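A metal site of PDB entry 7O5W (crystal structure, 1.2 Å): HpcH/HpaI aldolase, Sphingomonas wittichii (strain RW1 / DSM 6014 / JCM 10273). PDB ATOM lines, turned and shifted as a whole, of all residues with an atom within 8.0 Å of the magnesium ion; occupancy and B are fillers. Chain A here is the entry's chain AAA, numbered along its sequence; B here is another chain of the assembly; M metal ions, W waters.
The side-chain carboxylate (OD1) of Asp 172 lies within hydrogen-bond range of the backbone NH (N) of Phe 118 of chain B, at 2.8 Å. The side-chain carboxylate of Glu 146 lies within hydrogen-bond range of the backbone NH of Met 94 (2.8 Å). The side-chain amide nitrogen (NE2) of Gln 44 sits close to the side-chain hydroxyl (OG) of Ser 117 of chain B (3.5 Å). A ring nitrogen (NE2) of His 45 lies close to the side-chain hydroxyl (OG) of Ser 117 of chain B (2.7 Å). SD of Met 80 of chain B sits at hydrogen-bond distance from N of Ser 117 of chain B (3.4 Å). NE2 of His 45 lies close to OE1 of Gln 44, at 3.5 Å. The guanidinium group (NE) of Arg 70 lies close to the side-chain amide oxygen (OE1) of Gln 44 (3.2 Å).
Gln 44 touches the magnesium ion. Within 4 Å of the magnesium ion: Gln 44, Glu 146, Asp 172 and Ser 117 of chain B.
The magnesium ion is bound by OD2 of Asp 172. The magnesium ion is bound by OE1 of Glu 146 (2.0 Å). Water W1 binds the magnesium ion, 2.1 Å away. OG of Ser 117 of chain B is bound to the magnesium ion (2.1 Å). The magnesium ion is bound by water W2. Water W3 binds the magnesium ion.
Water W1 lies within hydrogen-bond range of the side-chain amide oxygen of Gln 44 (2.7 Å) and the guanidinium group of Arg 70 (3.4 Å). Water W3 bridges the side-chain carboxylate (OE2) of Glu 146 (2.6 Å) and the side-chain amide nitrogen (NE2) of Gln 44 (2.8 Å). Water W2 bridges the side-chain carboxylate (OD1) of Asp 172 and the side-chain sulfur (SD) of Met 94.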
ATOM      1  N   GLN A  44      16.020 -22.484  12.232  1.00  0.00           N
ATOM      2  CA  GLN A  44      15.442 -23.108  11.054  1.00  0.00           C
ATOM      3  C   GLN A  44      16.123 -22.545   9.788  1.00  0.00           C
ATOM      4  O   GLN A  44      16.781 -23.282   9.052  1.00  0.00           O
ATOM      5  CB  GLN A  44      13.929 -22.940  11.032  1.00  0.00           C
ATOM      6  CG  GLN A  44      13.271 -23.650   9.865  1.00  0.00           C
ATOM      7  CD  GLN A  44      11.778 -23.350   9.828  1.00  0.00           C
ATOM      8  OE1 GLN A  44      11.341 -22.225  10.054  1.00  0.00           O
ATOM      9  NE2 GLN A  44      11.000 -24.334   9.471  1.00  0.00           N
ATOM     10  N   HIS A  45      15.909 -21.277   9.498  1.00  0.00           N
ATOM     11  CA  HIS A  45      16.410 -20.646   8.240  1.00  0.00           C
ATOM     12  C   HIS A  45      17.661 -19.864   8.541  1.00  0.00           C
ATOM     13  O   HIS A  45      17.748 -18.629   8.397  1.00  0.00           O
ATOM     14  CB  HIS A  45      15.284 -19.807   7.605  1.00  0.00           C
ATOM     15  CG  HIS A  45      14.181 -20.682   7.127  1.00  0.00           C
ATOM     16  ND1 HIS A  45      14.382 -21.641   6.090  1.00  0.00           N
ATOM     17  CD2 HIS A  45      12.903 -20.853   7.484  1.00  0.00           C
ATOM     18  CE1 HIS A  45      13.239 -22.299   5.918  1.00  0.00           C
ATOM     19  NE2 HIS A  45      12.304 -21.854   6.761  1.00  0.00           N
ATOM     20  N   ARG A  70      13.212 -20.049  17.607  1.00  0.00           N
ATOM     21  CA  ARG A  70      12.337 -20.649  16.618  1.00  0.00           C
ATOM     22  C   ARG A  70      13.062 -21.886  16.134  1.00  0.00           C
ATOM     23  O   ARG A  70      14.151 -21.832  15.535  1.00  0.00           O
ATOM     24  CB  ARG A  70      12.002 -19.701  15.458  1.00  0.00           C
ATOM     25  CG  ARG A  70      10.973 -20.222  14.500  1.00  0.00           C
ATOM     26  CD  ARG A  70      11.525 -20.963  13.292  1.00  0.00           C
ATOM     27  NE  ARG A  70      12.130 -20.092  12.297  1.00  0.00           N
ATOM     28  CZ  ARG A  70      11.472 -19.451  11.373  1.00  0.00           C
ATOM     29  NH1 ARG A  70      10.145 -19.442  11.345  1.00  0.00           N
ATOM     30  NH2 ARG A  70      12.148 -18.766  10.466  1.00  0.00           N
ATOM     31  N   GLN A  72      13.873 -25.734  14.420  1.00  0.00           N
ATOM     32  CA  GLN A  72      13.762 -26.288  13.035  1.00  0.00           C
ATOM     33  C   GLN A  72      12.537 -27.156  12.901  1.00  0.00           C
ATOM     34  O   GLN A  72      12.066 -27.394  11.781  1.00  0.00           O
ATOM     35  CB  GLN A  72      14.971 -26.974  12.550  1.00  0.00           C
ATOM     36  CG  GLN A  72      15.129 -28.383  12.984  1.00  0.00           C
ATOM     37  CD  GLN A  72      16.343 -29.009  12.307  1.00  0.00           C
ATOM     38  OE1 GLN A  72      17.486 -28.547  12.451  1.00  0.00           O
ATOM     39  NE2 GLN A  72      16.102 -30.190  11.754  1.00  0.00           N
ATOM     40  N   PRO A  93       7.747 -24.645  14.308  1.00  0.00           N
ATOM     41  CA  PRO A  93       7.189 -24.636  12.958  1.00  0.00           C
ATOM     42  C   PRO A  93       6.188 -25.761  12.709  1.00  0.00           C
ATOM     43  O   PRO A  93       6.142 -26.788  13.353  1.00  0.00           O
ATOM     44  CB  PRO A  93       8.400 -24.883  12.069  1.00  0.00           C
ATOM     45  CG  PRO A  93       9.455 -25.363  12.904  1.00  0.00           C
ATOM     46  CD  PRO A  93       9.194 -24.982  14.336  1.00  0.00           C
ATOM     47  N   MET A  94       5.338 -25.492  11.696  1.00  0.00           N
ATOM     48  CA  MET A  94       4.462 -26.499  11.067  1.00  0.00           C
ATOM     49  C   MET A  94       3.568 -27.159  12.094  1.00  0.00           C
ATOM     50  O   MET A  94       3.353 -28.368  12.056  1.00  0.00           O
ATOM     51  CB  MET A  94       5.293 -27.553  10.315  1.00  0.00           C
ATOM     52  CG  MET A  94       5.985 -26.954   9.148  1.00  0.00           C
ATOM     53  SD  MET A  94       4.959 -26.186   7.850  1.00  0.00           S
ATOM     54  CE  MET A  94       4.572 -27.612   6.787  1.00  0.00           C
ATOM     55  N   MET A 144       3.547 -22.199  15.352  1.00  0.00           N
ATOM     56  CA  MET A 144       3.539 -21.502  14.050  1.00  0.00           C
ATOM     57  C   MET A 144       2.321 -21.890  13.235  1.00  0.00           C
ATOM     58  O   MET A 144       2.009 -23.068  13.089  1.00  0.00           O
ATOM     59  CB  MET A 144       4.756 -21.785  13.186  1.00  0.00           C
ATOM     60  CG  MET A 144       5.970 -21.100  13.650  1.00  0.00           C
ATOM     61  SD  MET A 144       7.400 -21.134  12.565  1.00  0.00           S
ATOM     62  CE  MET A 144       6.876 -20.109  11.190  1.00  0.00           C
ATOM     63  N   ILE A 145       1.737 -20.870  12.622  1.00  0.00           N
ATOM     64  CA  ILE A 145       0.656 -20.967  11.623  1.00  0.00           C
ATOM     65  C   ILE A 145       1.246 -20.496  10.305  1.00  0.00           C
ATOM     66  O   ILE A 145       1.485 -19.296  10.138  1.00  0.00           O
ATOM     67  CB  ILE A 145      -0.568 -20.161  12.049  1.00  0.00           C
ATOM     68  CG1 ILE A 145      -1.063 -20.551  13.436  1.00  0.00           C
ATOM     69  CG2 ILE A 145      -1.639 -20.240  10.983  1.00  0.00           C
ATOM     70  CD1 ILE A 145      -1.583 -21.963  13.574  1.00  0.00           C
ATOM     71  N   GLU A 146       1.465 -21.422   9.408  1.00  0.00           N
ATOM     72  CA  GLU A 146       2.226 -21.092   8.200  1.00  0.00           C
ATOM     73  C   GLU A 146       1.804 -21.966   7.029  1.00  0.00           C
ATOM     74  O   GLU A 146       2.503 -21.973   5.978  1.00  0.00           O
ATOM     75  CB  GLU A 146       3.739 -21.192   8.440  1.00  0.00           C
ATOM     76  CG  GLU A 146       4.204 -22.444   9.025  1.00  0.00           C
ATOM     77  CD  GLU A 146       5.683 -22.711   9.027  1.00  0.00           C
ATOM     78  OE1 GLU A 146       6.403 -22.090   8.232  1.00  0.00           O
ATOM     79  OE2 GLU A 146       6.086 -23.622   9.810  1.00  0.00           O
ATOM     80  N   THR A 147       0.629 -22.568   7.101  1.00  0.00           N
ATOM     81  CA  THR A 147       0.104 -23.391   6.028  1.00  0.00           C
ATOM     82  C   THR A 147      -1.404 -23.171   5.924  1.00  0.00           C
ATOM     83  O   THR A 147      -2.079 -22.747   6.904  1.00  0.00           O
ATOM     84  CB  THR A 147       0.337 -24.893   6.232  1.00  0.00           C
ATOM     85  OG1 THR A 147      -0.433 -25.306   7.352  1.00  0.00           O
ATOM     86  CG2 THR A 147       1.785 -25.266   6.396  1.00  0.00           C
ATOM     87  N   GLY A 169       3.740 -17.180  10.393  1.00  0.00           N
ATOM     88  CA  GLY A 169       4.856 -17.111   9.461  1.00  0.00           C
ATOM     89  C   GLY A 169       4.335 -16.701   8.109  1.00  0.00           C
ATOM     90  O   GLY A 169       3.852 -17.528   7.332  1.00  0.00           O
ATOM     91  N   THR A 171       5.431 -15.333   5.238  1.00  0.00           N
ATOM     92  CA  THR A 171       6.010 -15.649   3.919  1.00  0.00           C
ATOM     93  C   THR A 171       5.643 -17.050   3.514  1.00  0.00           C
ATOM     94  O   THR A 171       5.208 -17.289   2.384  1.00  0.00           O
ATOM     95  CB  THR A 171       7.517 -15.382   3.935  1.00  0.00           C
ATOM     96  OG1 THR A 171       8.184 -16.243   4.867  1.00  0.00           O
ATOM     97  CG2 THR A 171       7.802 -13.919   4.177  1.00  0.00           C
ATOM     98  N   ASP A 172       5.766 -17.982   4.467  1.00  0.00           N
ATOM     99  CA  ASP A 172       5.352 -19.377   4.204  1.00  0.00           C
ATOM    100  C   ASP A 172       3.856 -19.471   3.978  1.00  0.00           C
ATOM    101  O   ASP A 172       3.408 -20.213   3.107  1.00  0.00           O
ATOM    102  CB  ASP A 172       5.800 -20.338   5.283  1.00  0.00           C
ATOM    103  CG  ASP A 172       7.184 -20.898   5.022  1.00  0.00           C
ATOM    104  OD1 ASP A 172       7.528 -21.229   3.857  1.00  0.00           O
ATOM    105  OD2 ASP A 172       7.923 -21.000   6.043  1.00  0.00           O
ATOM    106  N   LEU A 173       3.054 -18.731   4.740  1.00  0.00           N
ATOM    107  CA  LEU A 173       1.600 -18.750   4.571  1.00  0.00           C
ATOM    108  C   LEU A 173       1.222 -18.233   3.162  1.00  0.00           C
ATOM    109  O   LEU A 173       0.431 -18.872   2.484  1.00  0.00           O
ATOM    110  CB  LEU A 173       0.953 -17.913   5.642  1.00  0.00           C
ATOM    111  CG  LEU A 173      -0.571 -17.990   5.633  1.00  0.00           C
ATOM    112  CD1 LEU A 173      -1.139 -19.418   5.766  1.00  0.00           C
ATOM    113  CD2 LEU A 173      -1.093 -17.034   6.731  1.00  0.00           C
ATOM    114  N   MET B  80      15.801 -29.678   4.832  1.00  0.00           N
ATOM    115  CA  MET B  80      15.561 -28.283   4.536  1.00  0.00           C
ATOM    116  C   MET B  80      16.690 -27.393   5.018  1.00  0.00           C
ATOM    117  O   MET B  80      17.083 -26.461   4.355  1.00  0.00           O
ATOM    118  CB  MET B  80      14.224 -27.851   5.152  1.00  0.00           C
ATOM    119  CG  MET B  80      13.043 -28.506   4.500  1.00  0.00           C
ATOM    120  SD  MET B  80      11.524 -27.974   5.333  1.00  0.00           S
ATOM    121  CE  MET B  80      10.455 -29.364   5.081  1.00  0.00           C
ATOM    122  N   LEU B 115       6.563 -29.352   0.575  1.00  0.00           N
ATOM    123  CA  LEU B 115       6.244 -28.527   1.766  1.00  0.00           C
ATOM    124  C   LEU B 115       7.492 -27.855   2.280  1.00  0.00           C
ATOM    125  O   LEU B 115       7.562 -27.417   3.448  1.00  0.00           O
ATOM    126  CB  LEU B 115       5.457 -29.259   2.823  1.00  0.00           C
ATOM    127  CG  LEU B 115       5.976 -30.600   3.230  1.00  0.00           C
ATOM    128  CD1 LEU B 115       7.392 -30.588   3.774  1.00  0.00           C
ATOM    129  CD2 LEU B 115       5.003 -31.331   4.118  1.00  0.00           C
ATOM    130  N   ARG B 116       8.553 -27.700   1.476  1.00  0.00           N
ATOM    131  CA  ARG B 116       9.788 -27.042   1.895  1.00  0.00           C
ATOM    132  C   ARG B 116       9.473 -25.667   2.460  1.00  0.00           C
ATOM    133  O   ARG B 116       8.811 -24.864   1.811  1.00  0.00           O
ATOM    134  CB  ARG B 116      10.742 -26.931   0.712  1.00  0.00           C
ATOM    135  CG  ARG B 116      12.088 -26.351   1.079  1.00  0.00           C
ATOM    136  CD  ARG B 116      13.009 -26.225  -0.102  1.00  0.00           C
ATOM    137  NE  ARG B 116      14.173 -25.500   0.226  1.00  0.00           N
ATOM    138  CZ  ARG B 116      15.026 -24.951  -0.640  1.00  0.00           C
ATOM    139  NH1 ARG B 116      14.842 -25.140  -1.936  1.00  0.00           N
ATOM    140  NH2 ARG B 116      16.058 -24.262  -0.221  1.00  0.00           N
ATOM    141  N   SER B 117      10.034 -25.392   3.620  1.00  0.00           N
ATOM    142  CA  SER B 117       9.844 -24.078   4.288  1.00  0.00           C
ATOM    143  C   SER B 117      10.744 -23.045   3.578  1.00  0.00           C
ATOM    144  O   SER B 117      11.870 -23.352   3.206  1.00  0.00           O
ATOM    145  CB  SER B 117      10.223 -24.221   5.719  1.00  0.00           C
ATOM    146  OG  SER B 117       9.955 -23.046   6.439  1.00  0.00           O
ATOM    147  N   PHE B 118      10.246 -21.845   3.441  1.00  0.00           N
ATOM    148  CA  PHE B 118      10.933 -20.762   2.724  1.00  0.00           C
ATOM    149  C   PHE B 118      11.804 -19.907   3.599  1.00  0.00           C
ATOM    150  O   PHE B 118      11.311 -19.165   4.463  1.00  0.00           O
ATOM    151  CB  PHE B 118       9.910 -19.878   1.989  1.00  0.00           C
ATOM    152  CG  PHE B 118      10.613 -18.941   1.020  1.00  0.00           C
ATOM    153  CD1 PHE B 118      11.007 -19.356  -0.231  1.00  0.00           C
ATOM    154  CD2 PHE B 118      10.867 -17.638   1.394  1.00  0.00           C
ATOM    155  CE1 PHE B 118      11.666 -18.511  -1.097  1.00  0.00           C
ATOM    156  CE2 PHE B 118      11.533 -16.764   0.523  1.00  0.00           C
ATOM    157  CZ  PHE B 118      11.965 -17.235  -0.687  1.00  0.00           C
ATOM    158  N   GLY B 119      13.115 -19.958   3.343  1.00  0.00           N
ATOM    159  CA  GLY B 119      14.110 -19.026   3.931  1.00  0.00           C
ATOM    160  C   GLY B 119      15.480 -19.424   3.435  1.00  0.00           C
ATOM    161  O   GLY B 119      16.321 -19.932   4.167  1.00  0.00           O
HETATM  162 MG    MG M   1       8.168 -22.511   7.346  1.00  0.00          MG
HETATM  163  O   HOH W   1       9.288 -21.285   8.566  1.00  0.00           O
HETATM  164  O   HOH W   2       7.161 -23.861   6.075  1.00  0.00           O
HETATM  165  O   HOH W   3       8.350 -24.158   8.662  1.00  0.00           O
